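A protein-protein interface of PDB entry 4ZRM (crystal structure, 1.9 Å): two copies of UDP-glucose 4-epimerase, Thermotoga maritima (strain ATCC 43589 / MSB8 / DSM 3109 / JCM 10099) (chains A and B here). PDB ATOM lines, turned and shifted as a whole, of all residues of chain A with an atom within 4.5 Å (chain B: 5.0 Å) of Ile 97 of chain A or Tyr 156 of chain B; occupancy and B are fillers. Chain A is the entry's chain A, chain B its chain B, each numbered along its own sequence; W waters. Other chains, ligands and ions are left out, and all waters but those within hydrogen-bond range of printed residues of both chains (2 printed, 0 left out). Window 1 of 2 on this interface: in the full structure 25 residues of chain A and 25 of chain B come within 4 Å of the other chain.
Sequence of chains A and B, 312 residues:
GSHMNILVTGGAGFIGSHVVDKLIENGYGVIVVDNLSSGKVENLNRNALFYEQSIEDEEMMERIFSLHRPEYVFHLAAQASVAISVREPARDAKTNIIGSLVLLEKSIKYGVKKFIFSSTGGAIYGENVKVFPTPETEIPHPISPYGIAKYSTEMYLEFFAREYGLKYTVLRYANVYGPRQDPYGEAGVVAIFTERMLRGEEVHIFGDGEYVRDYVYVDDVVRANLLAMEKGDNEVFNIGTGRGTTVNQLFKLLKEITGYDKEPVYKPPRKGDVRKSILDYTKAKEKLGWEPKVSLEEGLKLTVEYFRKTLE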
ATOM      1  N   ALA A  93      -9.410   0.410  13.533  1.00  0.00           N
ATOM      2  CA  ALA A  93      -8.764  -0.758  14.120  1.00  0.00           C
ATOM      3  C   ALA A  93      -9.200  -0.995  15.560  1.00  0.00           C
ATOM      4  O   ALA A  93      -9.247  -2.140  16.012  1.00  0.00           O
ATOM      5  CB  ALA A  93      -7.237  -0.632  14.034  1.00  0.00           C
ATOM      6  N   LYS A  94      -9.493   0.074  16.293  1.00  0.00           N
ATOM      7  CA  LYS A  94      -9.969  -0.083  17.669  1.00  0.00           C
ATOM      8  C   LYS A  94     -11.258  -0.890  17.689  1.00  0.00           C
ATOM      9  O   LYS A  94     -11.437  -1.765  18.530  1.00  0.00           O
ATOM     10  CB  LYS A  94     -10.212   1.272  18.334  1.00  0.00           C
ATOM     11  CG  LYS A  94      -8.954   2.054  18.688  1.00  0.00           C
ATOM     12  CD  LYS A  94      -9.349   3.314  19.471  1.00  0.00           C
ATOM     13  CE  LYS A  94      -8.140   4.146  19.848  1.00  0.00           C
ATOM     14  NZ  LYS A  94      -8.181   5.509  19.242  1.00  0.00           N
ATOM     15  N   THR A  95     -12.171  -0.581  16.777  1.00  0.00           N
ATOM     16  CA  THR A  95     -13.392  -1.371  16.675  1.00  0.00           C
ATOM     17  C   THR A  95     -13.127  -2.742  16.075  1.00  0.00           C
ATOM     18  O   THR A  95     -13.525  -3.772  16.639  1.00  0.00           O
ATOM     19  CB  THR A  95     -14.469  -0.651  15.824  1.00  0.00           C
ATOM     20  OG1 THR A  95     -14.948   0.478  16.554  1.00  0.00           O
ATOM     21  CG2 THR A  95     -15.652  -1.592  15.515  1.00  0.00           C
ATOM     22  N   ASN A  96     -12.462  -2.759  14.923  1.00  0.00           N
ATOM     23  CA  ASN A  96     -12.341  -3.992  14.153  1.00  0.00           C
ATOM     24  C   ASN A  96     -11.372  -5.015  14.740  1.00  0.00           C
ATOM     25  O   ASN A  96     -11.635  -6.215  14.682  1.00  0.00           O
ATOM     26  CB  ASN A  96     -12.023  -3.691  12.681  1.00  0.00           C
ATOM     27  CG  ASN A  96     -13.200  -3.065  11.965  1.00  0.00           C
ATOM     28  OD1 ASN A  96     -14.349  -3.246  12.385  1.00  0.00           O
ATOM     29  ND2 ASN A  96     -12.934  -2.311  10.901  1.00  0.00           N
ATOM     30  N   ILE A  97     -10.261  -4.559  15.313  1.00  0.00           N
ATOM     31  CA  ILE A  97      -9.324  -5.516  15.900  1.00  0.00           C
ATOM     32  C   ILE A  97      -9.464  -5.594  17.418  1.00  0.00           C
ATOM     33  O   ILE A  97      -9.683  -6.676  17.973  1.00  0.00           O
ATOM     34  CB  ILE A  97      -7.873  -5.182  15.553  1.00  0.00           C
ATOM     35  CG1 ILE A  97      -7.723  -5.020  14.037  1.00  0.00           C
ATOM     36  CG2 ILE A  97      -6.937  -6.294  16.056  1.00  0.00           C
ATOM     37  CD1 ILE A  97      -6.285  -4.660  13.620  1.00  0.00           C
ATOM     38  N   ILE A  98      -9.346  -4.462  18.099  1.00  0.00           N
ATOM     39  CA  ILE A  98      -9.385  -4.495  19.563  1.00  0.00           C
ATOM     40  C   ILE A  98     -10.741  -4.977  20.080  1.00  0.00           C
ATOM     41  O   ILE A  98     -10.804  -5.812  20.991  1.00  0.00           O
ATOM     42  CB  ILE A  98      -9.034  -3.129  20.199  1.00  0.00           C
ATOM     43  CG1 ILE A  98      -7.711  -2.604  19.637  1.00  0.00           C
ATOM     44  CG2 ILE A  98      -8.941  -3.258  21.717  1.00  0.00           C
ATOM     45  CD1 ILE A  98      -6.533  -3.555  19.827  1.00  0.00           C
ATOM     46  N   GLY A  99     -11.825  -4.468  19.497  1.00  0.00           N
ATOM     47  CA  GLY A  99     -13.156  -4.915  19.886  1.00  0.00           C
ATOM     48  C   GLY A  99     -13.309  -6.414  19.695  1.00  0.00           C
ATOM     49  O   GLY A  99     -13.870  -7.107  20.557  1.00  0.00           O
ATOM     50  N   SER A 100     -12.801  -6.936  18.582  1.00  0.00           N
ATOM     51  CA  SER A 100     -12.852  -8.385  18.357  1.00  0.00           C
ATOM     52  C   SER A 100     -12.085  -9.167  19.418  1.00  0.00           C
ATOM     53  O   SER A 100     -12.545 -10.223  19.885  1.00  0.00           O
ATOM     54  CB  SER A 100     -12.296  -8.728  16.978  1.00  0.00           C
ATOM     55  OG  SER A 100     -13.149  -8.237  15.962  1.00  0.00           O
ATOM     56  N   LEU A 101     -10.919  -8.653  19.800  1.00  0.00           N
ATOM     57  CA  LEU A 101     -10.085  -9.293  20.822  1.00  0.00           C
ATOM     58  C   LEU A 101     -10.719  -9.284  22.212  1.00  0.00           C
ATOM     59  O   LEU A 101     -10.590 -10.258  22.960  1.00  0.00           O
ATOM     60  CB  LEU A 101      -8.704  -8.633  20.874  1.00  0.00           C
ATOM     61  CG  LEU A 101      -7.867  -8.948  19.629  1.00  0.00           C
ATOM     62  CD1 LEU A 101      -6.550  -8.165  19.635  1.00  0.00           C
ATOM     63  CD2 LEU A 101      -7.596 -10.438  19.562  1.00  0.00           C
ATOM     64  N   PRO A 145      -7.296  -0.233   5.308  1.00  0.00           N
ATOM     65  CA  PRO A 145      -7.241  -0.518   6.745  1.00  0.00           C
ATOM     66  C   PRO A 145      -8.345  -1.482   7.164  1.00  0.00           C
ATOM     67  O   PRO A 145      -8.112  -2.369   7.985  1.00  0.00           O
ATOM     68  CB  PRO A 145      -7.434   0.867   7.368  1.00  0.00           C
ATOM     69  CG  PRO A 145      -6.806   1.795   6.354  1.00  0.00           C
ATOM     70  CD  PRO A 145      -7.287   1.217   5.038  1.00  0.00           C
ATOM     71  N   ILE A 148      -7.182  -5.002   6.121  1.00  0.00           N
ATOM     72  CA  ILE A 148      -6.091  -5.404   7.004  1.00  0.00           C
ATOM     73  C   ILE A 148      -6.620  -5.782   8.385  1.00  0.00           C
ATOM     74  O   ILE A 148      -6.210  -6.796   8.968  1.00  0.00           O
ATOM     75  CB  ILE A 148      -5.061  -4.278   7.156  1.00  0.00           C
ATOM     76  CG1 ILE A 148      -4.356  -4.037   5.808  1.00  0.00           C
ATOM     77  CG2 ILE A 148      -4.023  -4.658   8.216  1.00  0.00           C
ATOM     78  CD1 ILE A 148      -3.542  -2.734   5.762  1.00  0.00           C
ATOM     79  N   ALA A 149      -7.533  -4.973   8.910  1.00  0.00           N
ATOM     80  CA  ALA A 149      -8.143  -5.262  10.217  1.00  0.00           C
ATOM     81  C   ALA A 149      -8.882  -6.600  10.228  1.00  0.00           C
ATOM     82  O   ALA A 149      -8.754  -7.402  11.173  1.00  0.00           O
ATOM     83  CB  ALA A 149      -9.096  -4.132  10.619  1.00  0.00           C
ATOM     84  N   SER A 152      -6.323  -9.388  10.056  1.00  0.00           N
ATOM     85  CA  SER A 152      -5.684  -9.463  11.366  1.00  0.00           C
ATOM     86  C   SER A 152      -6.548 -10.264  12.330  1.00  0.00           C
ATOM     87  O   SER A 152      -6.066 -11.167  13.034  1.00  0.00           O
ATOM     88  CB  SER A 152      -5.472  -8.058  11.925  1.00  0.00           C
ATOM     89  OG  SER A 152      -4.643  -8.091  13.068  1.00  0.00           O
ATOM     90  N   THR A 153      -7.833  -9.939  12.359  1.00  0.00           N
ATOM     91  CA  THR A 153      -8.737 -10.610  13.271  1.00  0.00           C
ATOM     92  C   THR A 153      -8.860 -12.091  12.910  1.00  0.00           C
ATOM     93  O   THR A 153      -8.921 -12.927  13.809  1.00  0.00           O
ATOM     94  CB  THR A 153     -10.117  -9.909  13.309  1.00  0.00           C
ATOM     95  OG1 THR A 153      -9.942  -8.585  13.823  1.00  0.00           O
ATOM     96  CG2 THR A 153     -11.097 -10.677  14.204  1.00  0.00           C
ATOM     97  N   TYR A 156      -6.010 -13.805  14.531  1.00  0.00           N
ATOM     98  CA  TYR A 156      -6.202 -13.917  15.973  1.00  0.00           C
ATOM     99  C   TYR A 156      -7.151 -15.052  16.293  1.00  0.00           C
ATOM    100  O   TYR A 156      -6.979 -15.750  17.296  1.00  0.00           O
ATOM    101  CB  TYR A 156      -6.732 -12.620  16.585  1.00  0.00           C
ATOM    102  CG  TYR A 156      -5.669 -11.569  16.831  1.00  0.00           C
ATOM    103  CD1 TYR A 156      -5.689 -10.365  16.149  1.00  0.00           C
ATOM    104  CD2 TYR A 156      -4.646 -11.786  17.752  1.00  0.00           C
ATOM    105  CE1 TYR A 156      -4.720  -9.394  16.376  1.00  0.00           C
ATOM    106  CE2 TYR A 156      -3.674 -10.814  17.995  1.00  0.00           C
ATOM    107  CZ  TYR A 156      -3.720  -9.625  17.297  1.00  0.00           C
ATOM    108  OH  TYR A 156      -2.759  -8.655  17.520  1.00  0.00           O
ATOM    109  N   ALA B  93      -2.162  -5.817  21.478  1.00  0.00           N
ATOM    110  CA  ALA B  93      -2.574  -5.187  20.221  1.00  0.00           C
ATOM    111  C   ALA B  93      -2.781  -3.680  20.347  1.00  0.00           C
ATOM    112  O   ALA B  93      -2.555  -2.937  19.393  1.00  0.00           O
ATOM    113  CB  ALA B  93      -3.825  -5.859  19.663  1.00  0.00           C
ATOM    114  N   ILE B  97      -0.418  -2.517  17.585  1.00  0.00           N
ATOM    115  CA  ILE B  97      -1.112  -2.081  16.378  1.00  0.00           C
ATOM    116  C   ILE B  97      -1.657  -0.667  16.507  1.00  0.00           C
ATOM    117  O   ILE B  97      -1.315   0.209  15.708  1.00  0.00           O
ATOM    118  CB  ILE B  97      -2.275  -3.040  16.006  1.00  0.00           C
ATOM    119  CG1 ILE B  97      -1.764  -4.480  15.953  1.00  0.00           C
ATOM    120  CG2 ILE B  97      -2.902  -2.629  14.663  1.00  0.00           C
ATOM    121  CD1 ILE B  97      -2.847  -5.515  15.555  1.00  0.00           C
ATOM    122  N   LEU B 101      -0.453   2.786  14.586  1.00  0.00           N
ATOM    123  CA  LEU B 101      -1.391   3.517  13.733  1.00  0.00           C
ATOM    124  C   LEU B 101      -1.493   4.982  14.129  1.00  0.00           C
ATOM    125  O   LEU B 101      -1.578   5.859  13.257  1.00  0.00           O
ATOM    126  CB  LEU B 101      -2.778   2.851  13.747  1.00  0.00           C
ATOM    127  CG  LEU B 101      -2.852   1.505  13.017  1.00  0.00           C
ATOM    128  CD1 LEU B 101      -4.260   0.927  13.106  1.00  0.00           C
ATOM    129  CD2 LEU B 101      -2.451   1.649  11.546  1.00  0.00           C
ATOM    130  N   LEU B 104       1.584   6.621  12.778  1.00  0.00           N
ATOM    131  CA  LEU B 104       1.566   6.723  11.316  1.00  0.00           C
ATOM    132  C   LEU B 104       0.633   7.829  10.851  1.00  0.00           C
ATOM    133  O   LEU B 104       0.945   8.554   9.901  1.00  0.00           O
ATOM    134  CB  LEU B 104       1.182   5.381  10.686  1.00  0.00           C
ATOM    135  CG  LEU B 104       2.312   4.341  10.746  1.00  0.00           C
ATOM    136  CD1 LEU B 104       1.773   2.943  10.477  1.00  0.00           C
ATOM    137  CD2 LEU B 104       3.405   4.698   9.725  1.00  0.00           C
ATOM    138  N   SER B 152       0.536  -7.464  11.216  1.00  0.00           N
ATOM    139  CA  SER B 152      -0.550  -6.526  10.911  1.00  0.00           C
ATOM    140  C   SER B 152      -0.013  -5.117  10.694  1.00  0.00           C
ATOM    141  O   SER B 152      -0.397  -4.428   9.744  1.00  0.00           O
ATOM    142  CB  SER B 152      -1.607  -6.519  12.022  1.00  0.00           C
ATOM    143  OG  SER B 152      -2.183  -7.820  12.113  1.00  0.00           O
ATOM    144  N   THR B 153       0.884  -4.685  11.572  1.00  0.00           N
ATOM    145  CA  THR B 153       1.492  -3.362  11.423  1.00  0.00           C
ATOM    146  C   THR B 153       2.307  -3.229  10.136  1.00  0.00           C
ATOM    147  O   THR B 153       2.302  -2.169   9.499  1.00  0.00           O
ATOM    148  CB  THR B 153       2.339  -3.010  12.671  1.00  0.00           C
ATOM    149  OG1 THR B 153       1.471  -2.971  13.809  1.00  0.00           O
ATOM    150  CG2 THR B 153       2.998  -1.658  12.519  1.00  0.00           C
ATOM    151  N   GLU B 154       3.002  -4.293   9.735  1.00  0.00           N
ATOM    152  CA  GLU B 154       3.703  -4.265   8.454  1.00  0.00           C
ATOM    153  C   GLU B 154       2.740  -3.995   7.293  1.00  0.00           C
ATOM    154  O   GLU B 154       3.049  -3.216   6.375  1.00  0.00           O
ATOM    155  CB  GLU B 154       4.473  -5.574   8.202  1.00  0.00           C
ATOM    156  CG  GLU B 154       5.683  -5.823   9.134  1.00  0.00           C
ATOM    157  CD  GLU B 154       6.442  -7.106   8.765  1.00  0.00           C
ATOM    158  OE1 GLU B 154       6.127  -7.701   7.711  1.00  0.00           O
ATOM    159  OE2 GLU B 154       7.343  -7.544   9.519  1.00  0.00           O
ATOM    160  N   MET B 155       1.582  -4.645   7.311  1.00  0.00           N
ATOM    161  CA  MET B 155       0.595  -4.414   6.253  1.00  0.00           C
ATOM    162  C   MET B 155       0.076  -2.984   6.267  1.00  0.00           C
ATOM    163  O   MET B 155      -0.139  -2.374   5.213  1.00  0.00           O
ATOM    164  CB  MET B 155      -0.554  -5.425   6.342  1.00  0.00           C
ATOM    165  CG  MET B 155      -0.100  -6.838   6.005  1.00  0.00           C
ATOM    166  SD  MET B 155      -1.472  -8.009   6.001  1.00  0.00           S
ATOM    167  CE  MET B 155      -1.715  -8.197   7.764  1.00  0.00           C
ATOM    168  N   TYR B 156      -0.142  -2.445   7.456  1.00  0.00           N
ATOM    169  CA  TYR B 156      -0.587  -1.058   7.554  1.00  0.00           C
ATOM    170  C   TYR B 156       0.466  -0.103   6.994  1.00  0.00           C
ATOM    171  O   TYR B 156       0.127   0.902   6.364  1.00  0.00           O
ATOM    172  CB  TYR B 156      -0.909  -0.677   9.000  1.00  0.00           C
ATOM    173  CG  TYR B 156      -2.285  -1.107   9.490  1.00  0.00           C
ATOM    174  CD1 TYR B 156      -2.418  -2.031  10.513  1.00  0.00           C
ATOM    175  CD2 TYR B 156      -3.440  -0.560   8.940  1.00  0.00           C
ATOM    176  CE1 TYR B 156      -3.663  -2.408  10.981  1.00  0.00           C
ATOM    177  CE2 TYR B 156      -4.694  -0.925   9.394  1.00  0.00           C
ATOM    178  CZ  TYR B 156      -4.797  -1.855  10.412  1.00  0.00           C
ATOM    179  OH  TYR B 156      -6.033  -2.222  10.876  1.00  0.00           O
ATOM    180  N   LEU B 157       1.740  -0.399   7.237  1.00  0.00           N
ATOM    181  CA  LEU B 157       2.811   0.437   6.694  1.00  0.00           C
ATOM    182  C   LEU B 157       2.729   0.509   5.181  1.00  0.00           C
ATOM    183  O   LEU B 157       2.909   1.575   4.586  1.00  0.00           O
ATOM    184  CB  LEU B 157       4.180  -0.105   7.101  1.00  0.00           C
ATOM    185  CG  LEU B 157       4.717   0.330   8.444  1.00  0.00           C
ATOM    186  CD1 LEU B 157       5.972  -0.495   8.738  1.00  0.00           C
ATOM    187  CD2 LEU B 157       5.055   1.803   8.392  1.00  0.00           C
ATOM    188  N   GLU B 158       2.447  -0.621   4.549  1.00  0.00           N
ATOM    189  CA  GLU B 158       2.284  -0.640   3.105  1.00  0.00           C
ATOM    190  C   GLU B 158       1.105   0.224   2.668  1.00  0.00           C
ATOM    191  O   GLU B 158       1.183   0.905   1.645  1.00  0.00           O
ATOM    192  CB  GLU B 158       2.144  -2.074   2.573  1.00  0.00           C
ATOM    193  CG  GLU B 158       1.921  -2.159   1.067  1.00  0.00           C
ATOM    194  CD  GLU B 158       3.056  -1.554   0.230  1.00  0.00           C
ATOM    195  OE1 GLU B 158       4.242  -1.629   0.640  1.00  0.00           O
ATOM    196  OE2 GLU B 158       2.753  -1.005  -0.858  1.00  0.00           O
ATOM    197  N   PHE B 159       0.023   0.213   3.442  1.00  0.00           N
ATOM    198  CA  PHE B 159      -1.104   1.095   3.148  1.00  0.00           C
ATOM    199  C   PHE B 159      -0.692   2.569   3.194  1.00  0.00           C
ATOM    200  O   PHE B 159      -0.975   3.318   2.259  1.00  0.00           O
ATOM    201  CB  PHE B 159      -2.286   0.856   4.109  1.00  0.00           C
ATOM    202  CG  PHE B 159      -3.210   2.047   4.236  1.00  0.00           C
ATOM    203  CD1 PHE B 159      -4.121   2.337   3.229  1.00  0.00           C
ATOM    204  CD2 PHE B 159      -3.151   2.888   5.347  1.00  0.00           C
ATOM    205  CE1 PHE B 159      -4.963   3.444   3.319  1.00  0.00           C
ATOM    206  CE2 PHE B 159      -3.990   4.001   5.447  1.00  0.00           C
ATOM    207  CZ  PHE B 159      -4.899   4.277   4.430  1.00  0.00           C
ATOM    208  N   PHE B 160      -0.024   2.997   4.264  1.00  0.00           N
ATOM    209  CA  PHE B 160       0.347   4.419   4.358  1.00  0.00           C
ATOM    210  C   PHE B 160       1.288   4.838   3.233  1.00  0.00           C
ATOM    211  O   PHE B 160       1.209   5.972   2.746  1.00  0.00           O
ATOM    212  CB  PHE B 160       0.935   4.793   5.729  1.00  0.00           C
ATOM    213  CG  PHE B 160      -0.097   4.894   6.828  1.00  0.00           C
ATOM    214  CD1 PHE B 160      -0.720   6.108   7.109  1.00  0.00           C
ATOM    215  CD2 PHE B 160      -0.448   3.776   7.572  1.00  0.00           C
ATOM    216  CE1 PHE B 160      -1.674   6.202   8.118  1.00  0.00           C
ATOM    217  CE2 PHE B 160      -1.406   3.857   8.579  1.00  0.00           C
ATOM    218  CZ  PHE B 160      -2.015   5.071   8.858  1.00  0.00           C
HETATM  219  O   HOH W   1      -1.730  -8.776  20.092  1.00  0.00           O
HETATM  220  O   HOH W   2      -7.868  -0.255  10.562  1.00  0.00           O
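Ala 93 of chain A touches Leu 101 of chain B, and with the chains exchanged Leu 101 of chain A touches Ala 93 of chain B. Ala 93 of chain A touches Tyr 156 of chain B, and with the chains exchanged Tyr 156 of chain A touches Ala 93 of chain B. Ile 97 of chain A touches Tyr 156 of chain B, and with the chains exchanged Tyr 156 of chain A touches Ile 97 of chain B. Ser 152 of chain B touches its own counterpart, Ser 152 of chain A. 6 positions are printed for both chains. Of the 14 pairs that touch across the chains among the printed residues, 7 have their exchanged pair printed and touching as well.
The side-chain hydroxyl of Ser 152 of chain A is in hydrogen-bond range of the side-chain hydroxyl of Ser 152 of chain B (2.7 Å).
Ile 97 of chain A touches just one residue of chain B: Tyr 156. Printed residues of chain A within 4 Å of Ser 152 of chain B: Ile 148 and Ser 152. Printed residues of chain A within 4 Å of Leu 101 of chain B: Ala 93. Of the printed residues of chain B, Ile 98 of chain A touches Ala 93. The nearest residue of chain B that does not touch Ile 97 of chain A is Ile 97 of chain B (4.04 Å). The nearest printed residue of chain A that does not touch Tyr 156 of chain B is Ser 152 of chain A (6.0 Å).
Water W2 lies within hydrogen-bond range of the side-chain hydroxyl of Tyr 156 of chain B (2.7 Å), the backbone carbonyl oxygen of Pro 145 of chain A (3.3 Å) and the backbone NH of Ala 93 of chain A (3.4 Å). Water W1 lies within hydrogen-bond range of OH of Tyr 156 of chain A (2.8 Å) and N of Ala 93 of chain B (3.3 Å).
Printed residues of chain B that touch a printed residue of chain A: Ala 93, Ile 97, Leu 101, Ser 152, Met 155, Tyr 156 and Phe 159. Among the printed residues, no Asp or Glu carboxylate lies within 4 Å of a Lys or Arg side-chain nitrogen of the other chain.
O of Ala 93 of chain A lies within hydrogen-bond range of N of Ile 98 of chain A. The side-chain hydroxyl of Thr 153 of chain A is in hydrogen-bond range of the backbone carbonyl oxygen of Ala 149 of chain A (3.1 Å).
Among the printed residues, pairs that only touch across the chains: Ala 93 of chain A with Leu 101 of chain B (3.5 Å), Ala 93 of chain A with Tyr 156 of chain B (3.7 Å), Ile 97 of chain A with Tyr 156 of chain B (3.7 Å), Ile 98 of chain A with Ala 93 of chain B (3.6 Å), Leu 101 of chain A with Ala 93 of chain B (3.6 Å), Pro 145 of chain A with Tyr 156 of chain B (3.6 Å), Pro 145 of chain A with Phe 159 of chain B (3.6 Å), Ile 148 of chain A with Ser 152 of chain B (3.9 Å), Ile 148 of chain A with Met 155 of chain B (3.5 Å), Ile 148 of chain A with Tyr 156 of chain B (3.6 Å), Ala 149 of chain A with Tyr 156 of chain B (3.6 Å), Tyr 156 of chain A with Ala 93 of chain B (3.7 Å) and Tyr 156 of chain A with Ile 97 of chain B (3.7 Å).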
